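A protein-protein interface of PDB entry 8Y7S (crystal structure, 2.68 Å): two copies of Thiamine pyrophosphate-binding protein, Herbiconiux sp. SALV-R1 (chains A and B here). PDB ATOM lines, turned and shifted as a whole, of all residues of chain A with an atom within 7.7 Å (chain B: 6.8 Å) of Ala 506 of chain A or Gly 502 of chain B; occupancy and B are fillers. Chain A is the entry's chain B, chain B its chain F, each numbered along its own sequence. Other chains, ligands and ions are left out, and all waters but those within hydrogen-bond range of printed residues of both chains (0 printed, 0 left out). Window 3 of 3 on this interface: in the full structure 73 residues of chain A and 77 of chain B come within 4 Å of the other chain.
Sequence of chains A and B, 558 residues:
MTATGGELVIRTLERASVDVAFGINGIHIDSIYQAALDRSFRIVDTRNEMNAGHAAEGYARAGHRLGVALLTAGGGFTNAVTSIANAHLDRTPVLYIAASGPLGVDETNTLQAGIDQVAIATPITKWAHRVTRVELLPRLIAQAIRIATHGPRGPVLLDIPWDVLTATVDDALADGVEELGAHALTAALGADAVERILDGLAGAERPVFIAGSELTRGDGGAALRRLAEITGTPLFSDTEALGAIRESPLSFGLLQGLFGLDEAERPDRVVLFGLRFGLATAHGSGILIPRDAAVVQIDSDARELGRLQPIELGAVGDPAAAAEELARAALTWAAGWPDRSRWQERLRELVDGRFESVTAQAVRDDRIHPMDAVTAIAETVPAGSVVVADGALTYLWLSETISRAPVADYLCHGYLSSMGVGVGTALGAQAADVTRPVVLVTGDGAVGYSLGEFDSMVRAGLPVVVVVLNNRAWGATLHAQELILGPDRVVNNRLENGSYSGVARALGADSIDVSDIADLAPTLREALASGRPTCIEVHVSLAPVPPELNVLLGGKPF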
ATOM      1  N   PHE A 454      23.773  17.535   4.773  1.00  0.00           N
ATOM      2  CA  PHE A 454      24.902  16.677   4.432  1.00  0.00           C
ATOM      3  C   PHE A 454      25.106  16.613   2.925  1.00  0.00           C
ATOM      4  O   PHE A 454      26.245  16.636   2.443  1.00  0.00           O
ATOM      5  CB  PHE A 454      24.692  15.275   5.004  1.00  0.00           C
ATOM      6  CG  PHE A 454      24.986  15.169   6.473  1.00  0.00           C
ATOM      7  CD1 PHE A 454      26.250  15.457   6.964  1.00  0.00           C
ATOM      8  CD2 PHE A 454      23.996  14.788   7.366  1.00  0.00           C
ATOM      9  CE1 PHE A 454      26.521  15.363   8.317  1.00  0.00           C
ATOM     10  CE2 PHE A 454      24.263  14.693   8.717  1.00  0.00           C
ATOM     11  CZ  PHE A 454      25.525  14.986   9.195  1.00  0.00           C
ATOM     12  N   ASP A 455      24.013  16.549   2.161  1.00  0.00           N
ATOM     13  CA  ASP A 455      24.122  16.581   0.708  1.00  0.00           C
ATOM     14  C   ASP A 455      24.734  17.891   0.220  1.00  0.00           C
ATOM     15  O   ASP A 455      25.561  17.887  -0.701  1.00  0.00           O
ATOM     16  CB  ASP A 455      22.751  16.359   0.073  1.00  0.00           C
ATOM     17  CG  ASP A 455      22.699  16.823  -1.368  1.00  0.00           C
ATOM     18  OD1 ASP A 455      22.191  17.935  -1.626  1.00  0.00           O
ATOM     19  OD2 ASP A 455      23.200  16.085  -2.243  1.00  0.00           O
ATOM     20  N   SER A 499      19.270   6.256  12.816  1.00  0.00           N
ATOM     21  CA  SER A 499      20.730   6.307  12.793  1.00  0.00           C
ATOM     22  C   SER A 499      21.155   7.536  11.993  1.00  0.00           C
ATOM     23  O   SER A 499      20.853   7.639  10.798  1.00  0.00           O
ATOM     24  CB  SER A 499      21.309   5.024  12.196  1.00  0.00           C
ATOM     25  OG  SER A 499      22.691   5.155  11.915  1.00  0.00           O
ATOM     26  N   TYR A 500      21.797   8.498  12.658  1.00  0.00           N
ATOM     27  CA  TYR A 500      22.222   9.714  11.962  1.00  0.00           C
ATOM     28  C   TYR A 500      23.436   9.461  11.077  1.00  0.00           C
ATOM     29  O   TYR A 500      23.546  10.033   9.985  1.00  0.00           O
ATOM     30  CB  TYR A 500      22.480  10.809  12.988  1.00  0.00           C
ATOM     31  CG  TYR A 500      21.259  11.001  13.836  1.00  0.00           C
ATOM     32  CD1 TYR A 500      20.107  11.561  13.297  1.00  0.00           C
ATOM     33  CD2 TYR A 500      21.218  10.542  15.145  1.00  0.00           C
ATOM     34  CE1 TYR A 500      18.964  11.711  14.053  1.00  0.00           C
ATOM     35  CE2 TYR A 500      20.073  10.687  15.915  1.00  0.00           C
ATOM     36  CZ  TYR A 500      18.950  11.273  15.360  1.00  0.00           C
ATOM     37  OH  TYR A 500      17.806  11.422  16.097  1.00  0.00           O
ATOM     38  N   SER A 501      24.347   8.594  11.524  1.00  0.00           N
ATOM     39  CA  SER A 501      25.418   8.136  10.647  1.00  0.00           C
ATOM     40  C   SER A 501      24.835   7.470   9.414  1.00  0.00           C
ATOM     41  O   SER A 501      25.353   7.632   8.301  1.00  0.00           O
ATOM     42  CB  SER A 501      26.335   7.171  11.393  1.00  0.00           C
ATOM     43  OG  SER A 501      25.689   5.927  11.615  1.00  0.00           O
ATOM     44  N   GLY A 502      23.760   6.705   9.598  1.00  0.00           N
ATOM     45  CA  GLY A 502      23.090   6.104   8.460  1.00  0.00           C
ATOM     46  C   GLY A 502      22.579   7.134   7.474  1.00  0.00           C
ATOM     47  O   GLY A 502      22.733   6.981   6.260  1.00  0.00           O
ATOM     48  N   VAL A 503      21.934   8.187   7.980  1.00  0.00           N
ATOM     49  CA  VAL A 503      21.394   9.217   7.097  1.00  0.00           C
ATOM     50  C   VAL A 503      22.517   9.929   6.348  1.00  0.00           C
ATOM     51  O   VAL A 503      22.453  10.120   5.125  1.00  0.00           O
ATOM     52  CB  VAL A 503      20.526  10.201   7.895  1.00  0.00           C
ATOM     53  CG1 VAL A 503      20.033  11.326   6.985  1.00  0.00           C
ATOM     54  CG2 VAL A 503      19.358   9.460   8.534  1.00  0.00           C
ATOM     55  N   ALA A 504      23.566  10.325   7.068  1.00  0.00           N
ATOM     56  CA  ALA A 504      24.660  11.045   6.429  1.00  0.00           C
ATOM     57  C   ALA A 504      25.339  10.194   5.356  1.00  0.00           C
ATOM     58  O   ALA A 504      25.680  10.701   4.281  1.00  0.00           O
ATOM     59  CB  ALA A 504      25.658  11.515   7.484  1.00  0.00           C
ATOM     60  N   ARG A 505      25.553   8.901   5.633  1.00  0.00           N
ATOM     61  CA  ARG A 505      26.147   8.009   4.637  1.00  0.00           C
ATOM     62  C   ARG A 505      25.292   7.940   3.381  1.00  0.00           C
ATOM     63  O   ARG A 505      25.807   8.016   2.259  1.00  0.00           O
ATOM     64  CB  ARG A 505      26.339   6.610   5.227  1.00  0.00           C
ATOM     65  CG  ARG A 505      27.087   5.638   4.315  1.00  0.00           C
ATOM     66  CD  ARG A 505      26.901   4.197   4.778  1.00  0.00           C
ATOM     67  NE  ARG A 505      26.987   4.077   6.229  1.00  0.00           N
ATOM     68  CZ  ARG A 505      26.029   3.579   7.004  1.00  0.00           C
ATOM     69  NH1 ARG A 505      24.891   3.127   6.499  1.00  0.00           N
ATOM     70  NH2 ARG A 505      26.216   3.542   8.321  1.00  0.00           N
ATOM     71  N   ALA A 506      23.974   7.792   3.548  1.00  0.00           N
ATOM     72  CA  ALA A 506      23.080   7.753   2.396  1.00  0.00           C
ATOM     73  C   ALA A 506      23.132   9.052   1.607  1.00  0.00           C
ATOM     74  O   ALA A 506      22.821   9.059   0.409  1.00  0.00           O
ATOM     75  CB  ALA A 506      21.649   7.464   2.846  1.00  0.00           C
ATOM     76  N   LEU A 507      23.521  10.149   2.254  1.00  0.00           N
ATOM     77  CA  LEU A 507      23.673  11.440   1.602  1.00  0.00           C
ATOM     78  C   LEU A 507      25.093  11.681   1.098  1.00  0.00           C
ATOM     79  O   LEU A 507      25.396  12.790   0.650  1.00  0.00           O
ATOM     80  CB  LEU A 507      23.237  12.561   2.551  1.00  0.00           C
ATOM     81  CG  LEU A 507      21.734  12.526   2.838  1.00  0.00           C
ATOM     82  CD1 LEU A 507      21.297  13.629   3.791  1.00  0.00           C
ATOM     83  CD2 LEU A 507      20.955  12.592   1.524  1.00  0.00           C
ATOM     84  N   GLY A 508      25.961  10.676   1.157  1.00  0.00           N
ATOM     85  CA  GLY A 508      27.263  10.754   0.527  1.00  0.00           C
ATOM     86  C   GLY A 508      28.404  11.223   1.398  1.00  0.00           C
ATOM     87  O   GLY A 508      29.484  11.510   0.869  1.00  0.00           O
ATOM     88  N   ALA A 509      28.220  11.292   2.703  1.00  0.00           N
ATOM     89  CA  ALA A 509      29.255  11.769   3.605  1.00  0.00           C
ATOM     90  C   ALA A 509      29.943  10.610   4.316  1.00  0.00           C
ATOM     91  O   ALA A 509      29.414   9.499   4.400  1.00  0.00           O
ATOM     92  CB  ALA A 509      28.664  12.733   4.637  1.00  0.00           C
ATOM     93  N   SER A 511      30.739   8.598   7.458  1.00  0.00           N
ATOM     94  CA  SER A 511      29.926   8.365   8.645  1.00  0.00           C
ATOM     95  C   SER A 511      30.548   7.258   9.484  1.00  0.00           C
ATOM     96  O   SER A 511      30.962   6.224   8.954  1.00  0.00           O
ATOM     97  CB  SER A 511      28.479   8.013   8.273  1.00  0.00           C
ATOM     98  OG  SER A 511      28.378   6.677   7.811  1.00  0.00           O
ATOM     99  N   ASN B 497      23.127  13.610  -6.222  1.00  0.00           N
ATOM    100  CA  ASN B 497      23.777  13.020  -5.061  1.00  0.00           C
ATOM    101  C   ASN B 497      22.709  12.494  -4.111  1.00  0.00           C
ATOM    102  O   ASN B 497      21.591  13.004  -4.079  1.00  0.00           O
ATOM    103  CB  ASN B 497      24.671  14.056  -4.367  1.00  0.00           C
ATOM    104  CG  ASN B 497      25.252  13.557  -3.067  1.00  0.00           C
ATOM    105  OD1 ASN B 497      26.068  12.636  -3.053  1.00  0.00           O
ATOM    106  ND2 ASN B 497      24.840  14.165  -1.962  1.00  0.00           N
ATOM    107  N   GLY B 498      23.058  11.454  -3.362  1.00  0.00           N
ATOM    108  CA  GLY B 498      22.251  11.027  -2.226  1.00  0.00           C
ATOM    109  C   GLY B 498      21.156  10.044  -2.593  1.00  0.00           C
ATOM    110  O   GLY B 498      20.636  10.020  -3.712  1.00  0.00           O
ATOM    111  N   SER B 499      20.803   9.206  -1.619  1.00  0.00           N
ATOM    112  CA  SER B 499      19.723   8.233  -1.745  1.00  0.00           C
ATOM    113  C   SER B 499      18.662   8.542  -0.699  1.00  0.00           C
ATOM    114  O   SER B 499      18.904   8.379   0.502  1.00  0.00           O
ATOM    115  CB  SER B 499      20.247   6.809  -1.574  1.00  0.00           C
ATOM    116  OG  SER B 499      19.212   5.929  -1.165  1.00  0.00           O
ATOM    117  N   TYR B 500      17.488   8.987  -1.152  1.00  0.00           N
ATOM    118  CA  TYR B 500      16.408   9.294  -0.218  1.00  0.00           C
ATOM    119  C   TYR B 500      15.803   8.026   0.365  1.00  0.00           C
ATOM    120  O   TYR B 500      15.380   8.021   1.527  1.00  0.00           O
ATOM    121  CB  TYR B 500      15.359  10.151  -0.913  1.00  0.00           C
ATOM    122  CG  TYR B 500      15.993  11.358  -1.561  1.00  0.00           C
ATOM    123  CD1 TYR B 500      16.437  12.432  -0.792  1.00  0.00           C
ATOM    124  CD2 TYR B 500      16.197  11.406  -2.934  1.00  0.00           C
ATOM    125  CE1 TYR B 500      17.036  13.526  -1.375  1.00  0.00           C
ATOM    126  CE2 TYR B 500      16.795  12.497  -3.524  1.00  0.00           C
ATOM    127  CZ  TYR B 500      17.213  13.554  -2.743  1.00  0.00           C
ATOM    128  OH  TYR B 500      17.809  14.637  -3.350  1.00  0.00           O
ATOM    129  N   SER B 501      15.755   6.949  -0.425  1.00  0.00           N
ATOM    130  CA  SER B 501      15.406   5.644   0.125  1.00  0.00           C
ATOM    131  C   SER B 501      16.395   5.232   1.206  1.00  0.00           C
ATOM    132  O   SER B 501      16.001   4.706   2.254  1.00  0.00           O
ATOM    133  CB  SER B 501      15.368   4.598  -0.990  1.00  0.00           C
ATOM    134  OG  SER B 501      16.514   4.692  -1.815  1.00  0.00           O
ATOM    135  N   GLY B 502      17.685   5.470   0.971  1.00  0.00           N
ATOM    136  CA  GLY B 502      18.677   5.189   1.996  1.00  0.00           C
ATOM    137  C   GLY B 502      18.431   5.971   3.270  1.00  0.00           C
ATOM    138  O   GLY B 502      18.512   5.422   4.370  1.00  0.00           O
ATOM    139  N   VAL B 503      18.116   7.265   3.133  1.00  0.00           N
ATOM    140  CA  VAL B 503      17.867   8.128   4.290  1.00  0.00           C
ATOM    141  C   VAL B 503      16.684   7.608   5.104  1.00  0.00           C
ATOM    142  O   VAL B 503      16.743   7.522   6.338  1.00  0.00           O
ATOM    143  CB  VAL B 503      17.635   9.576   3.823  1.00  0.00           C
ATOM    144  CG1 VAL B 503      17.043  10.426   4.940  1.00  0.00           C
ATOM    145  CG2 VAL B 503      18.928  10.183   3.309  1.00  0.00           C
ATOM    146  N   ALA B 504      15.593   7.257   4.421  1.00  0.00           N
ATOM    147  CA  ALA B 504      14.402   6.774   5.112  1.00  0.00           C
ATOM    148  C   ALA B 504      14.690   5.498   5.887  1.00  0.00           C
ATOM    149  O   ALA B 504      14.224   5.335   7.021  1.00  0.00           O
ATOM    150  CB  ALA B 504      13.272   6.550   4.110  1.00  0.00           C
ATOM    151  N   ARG B 505      15.451   4.576   5.286  1.00  0.00           N
ATOM    152  CA  ARG B 505      15.796   3.331   5.966  1.00  0.00           C
ATOM    153  C   ARG B 505      16.546   3.603   7.259  1.00  0.00           C
ATOM    154  O   ARG B 505      16.251   3.004   8.298  1.00  0.00           O
ATOM    155  CB  ARG B 505      16.634   2.444   5.042  1.00  0.00           C
ATOM    156  CG  ARG B 505      16.274   0.967   5.092  1.00  0.00           C
ATOM    157  CD  ARG B 505      17.150   0.153   4.169  1.00  0.00           C
ATOM    158  NE  ARG B 505      16.493  -0.079   2.888  1.00  0.00           N
ATOM    159  CZ  ARG B 505      16.902   0.427   1.731  1.00  0.00           C
ATOM    160  NH1 ARG B 505      17.994   1.172   1.647  1.00  0.00           N
ATOM    161  NH2 ARG B 505      16.200   0.178   0.628  1.00  0.00           N
ATOM    162  N   ALA B 506      17.527   4.508   7.214  1.00  0.00           N
ATOM    163  CA  ALA B 506      18.288   4.833   8.411  1.00  0.00           C
ATOM    164  C   ALA B 506      17.410   5.445   9.502  1.00  0.00           C
ATOM    165  O   ALA B 506      17.771   5.382  10.686  1.00  0.00           O
ATOM    166  CB  ALA B 506      19.450   5.760   8.060  1.00  0.00           C
ATOM    167  N   LEU B 507      16.275   6.043   9.134  1.00  0.00           N
ATOM    168  CA  LEU B 507      15.335   6.594  10.101  1.00  0.00           C
ATOM    169  C   LEU B 507      14.235   5.606  10.490  1.00  0.00           C
ATOM    170  O   LEU B 507      13.321   5.973  11.237  1.00  0.00           O
ATOM    171  CB  LEU B 507      14.721   7.881   9.553  1.00  0.00           C
ATOM    172  CG  LEU B 507      15.722   9.034   9.455  1.00  0.00           C
ATOM    173  CD1 LEU B 507      15.067  10.279   8.872  1.00  0.00           C
ATOM    174  CD2 LEU B 507      16.346   9.329  10.817  1.00  0.00           C
ATOM    175  N   SER B 511      11.755   1.146   2.839  1.00  0.00           N
ATOM    176  CA  SER B 511      12.442   1.824   1.748  1.00  0.00           C
ATOM    177  C   SER B 511      12.594   0.905   0.549  1.00  0.00           C
ATOM    178  O   SER B 511      12.967  -0.262   0.688  1.00  0.00           O
ATOM    179  CB  SER B 511      13.829   2.303   2.183  1.00  0.00           C
ATOM    180  OG  SER B 511      13.791   2.795   3.508  1.00  0.00           O
ATOM    181  N   ASP B 513      13.582   1.227  -3.971  1.00  0.00           N
ATOM    182  CA  ASP B 513      13.907   1.972  -5.185  1.00  0.00           C
ATOM    183  C   ASP B 513      13.189   1.346  -6.371  1.00  0.00           C
ATOM    184  O   ASP B 513      13.067   0.121  -6.451  1.00  0.00           O
ATOM    185  CB  ASP B 513      15.408   1.987  -5.469  1.00  0.00           C
ATOM    186  CG  ASP B 513      16.176   2.857  -4.511  1.00  0.00           C
ATOM    187  OD1 ASP B 513      16.269   2.492  -3.321  1.00  0.00           O
ATOM    188  OD2 ASP B 513      16.704   3.896  -4.952  1.00  0.00           O
ATOM    189  N   CYS B 535       9.078   4.827   1.995  1.00  0.00           N
ATOM    190  CA  CYS B 535       9.631   5.739   1.005  1.00  0.00           C
ATOM    191  C   CYS B 535       9.939   4.951  -0.258  1.00  0.00           C
ATOM    192  O   CYS B 535      10.688   3.969  -0.219  1.00  0.00           O
ATOM    193  CB  CYS B 535      10.890   6.438   1.519  1.00  0.00           C
ATOM    194  SG  CYS B 535      11.826   7.277   0.202  1.00  0.00           S
ATOM    195  N   GLU B 537      11.573   5.531  -3.807  1.00  0.00           N
ATOM    196  CA  GLU B 537      12.363   6.423  -4.650  1.00  0.00           C
ATOM    197  C   GLU B 537      12.213   5.974  -6.095  1.00  0.00           C
ATOM    198  O   GLU B 537      12.679   4.895  -6.469  1.00  0.00           O
ATOM    199  CB  GLU B 537      13.834   6.439  -4.239  1.00  0.00           C
ATOM    200  CG  GLU B 537      14.639   7.479  -5.017  1.00  0.00           C
ATOM    201  CD  GLU B 537      15.962   7.830  -4.361  1.00  0.00           C
ATOM    202  OE1 GLU B 537      16.145   7.510  -3.167  1.00  0.00           O
ATOM    203  OE2 GLU B 537      16.821   8.433  -5.044  1.00  0.00           O
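The side-chain carboxylate of Asp 455 of chain A is in hydrogen-bond range of the side-chain amide nitrogen of Asn 497 of chain B (2.5 Å). The backbone carbonyl oxygen of Ala 506 of chain B is in hydrogen-bond range of the backbone NH of Ser 499 of chain A (2.7 Å). The backbone NH of Ser 499 of chain B lies within hydrogen-bond range of the backbone carbonyl oxygen of Ala 506 of chain A (2.9 Å). The backbone carbonyl oxygen (O) of Leu 507 of chain A is in hydrogen-bond range of the side-chain amide nitrogen (ND2) of Asn 497 of chain B.
The side-chain hydroxyl (OG) of Ser 499 of chain A sits at hydrogen-bond distance from the side-chain hydroxyl (OG) of Ser 501 of chain A. N of Gly 502 of chain A sits at hydrogen-bond distance from OG of Ser 499 of chain A. OG of Ser 501 of chain B is in hydrogen-bond range of OG of Ser 499 of chain B, at 3.0 Å. The backbone NH of Gly 502 of chain B sits at hydrogen-bond distance from the side-chain hydroxyl of Ser 499 of chain B (2.7 Å).
Among the printed residues, pairs that only touch across the chains: Ala 506 of chain A with Gly 498 of chain B, Gly 502 of chain A with Ala 506 of chain B, Val 503 of chain A with Ala 506 of chain B, Ala 506 of chain A with Val 503 of chain B, Ala 506 of chain A with Gly 502 of chain B, Leu 507 of chain A with Val 503 of chain B, Val 503 of chain A with Val 503 of chain B and Val 503 of chain A with Leu 507 of chain B.
Ala 504 of chain A touches none of the printed residues of chain B. Printed residues of chain B within 4 Å of Leu 507 of chain A: Asn 497 (3.0 Å) and Val 503 (3.6 Å). Gly 502 of chain B touches one residue of chain A. Printed residues of chain A within 4 Å of Ala 506 of chain B: Ser 499 (2.7 Å), Gly 502 (3.5 Å) and Val 503 (3.5 Å). The nearest residue of chain A that does not touch Gly 502 of chain B is Gly 502 of chain A (4.9 Å).
Of the 14 printed residues of chain A, 6 touch a printed residue of chain B. Hydrophobic or aromatic side chains of chain A that line the printed part of chain B: Val 503, Ala 506 and Leu 507. Of the 15 printed residues of chain B, 7 touch a printed residue of chain A. Printed residues of chain B that touch a printed residue of chain A: Asn 497, Gly 498, Ser 499, Gly 502, Val 503, Ala 506 and Leu 507. Hydrophobic or aromatic side chains of chain B that line the printed part of chain A: Val 503, Ala 506 and Leu 507. Along chain B the printed residues that touch a printed residue of chain A span positions 497 to 507.
Ser 499 of chain A touches Ala 506 of chain B, and with the chains exchanged Ala 506 of chain A touches Ser 499 of chain B. Gly 502 of chain A touches Ala 506 of chain B, and with the chains exchanged Ala 506 of chain A touches Gly 502 of chain B. Val 503 of chain B touches its own counterpart, Val 503 of chain A. Val 503 of chain A touches Ala 506 of chain B, and with the chains exchanged Ala 506 of chain A touches Val 503 of chain B. 10 positions are printed for both chains.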
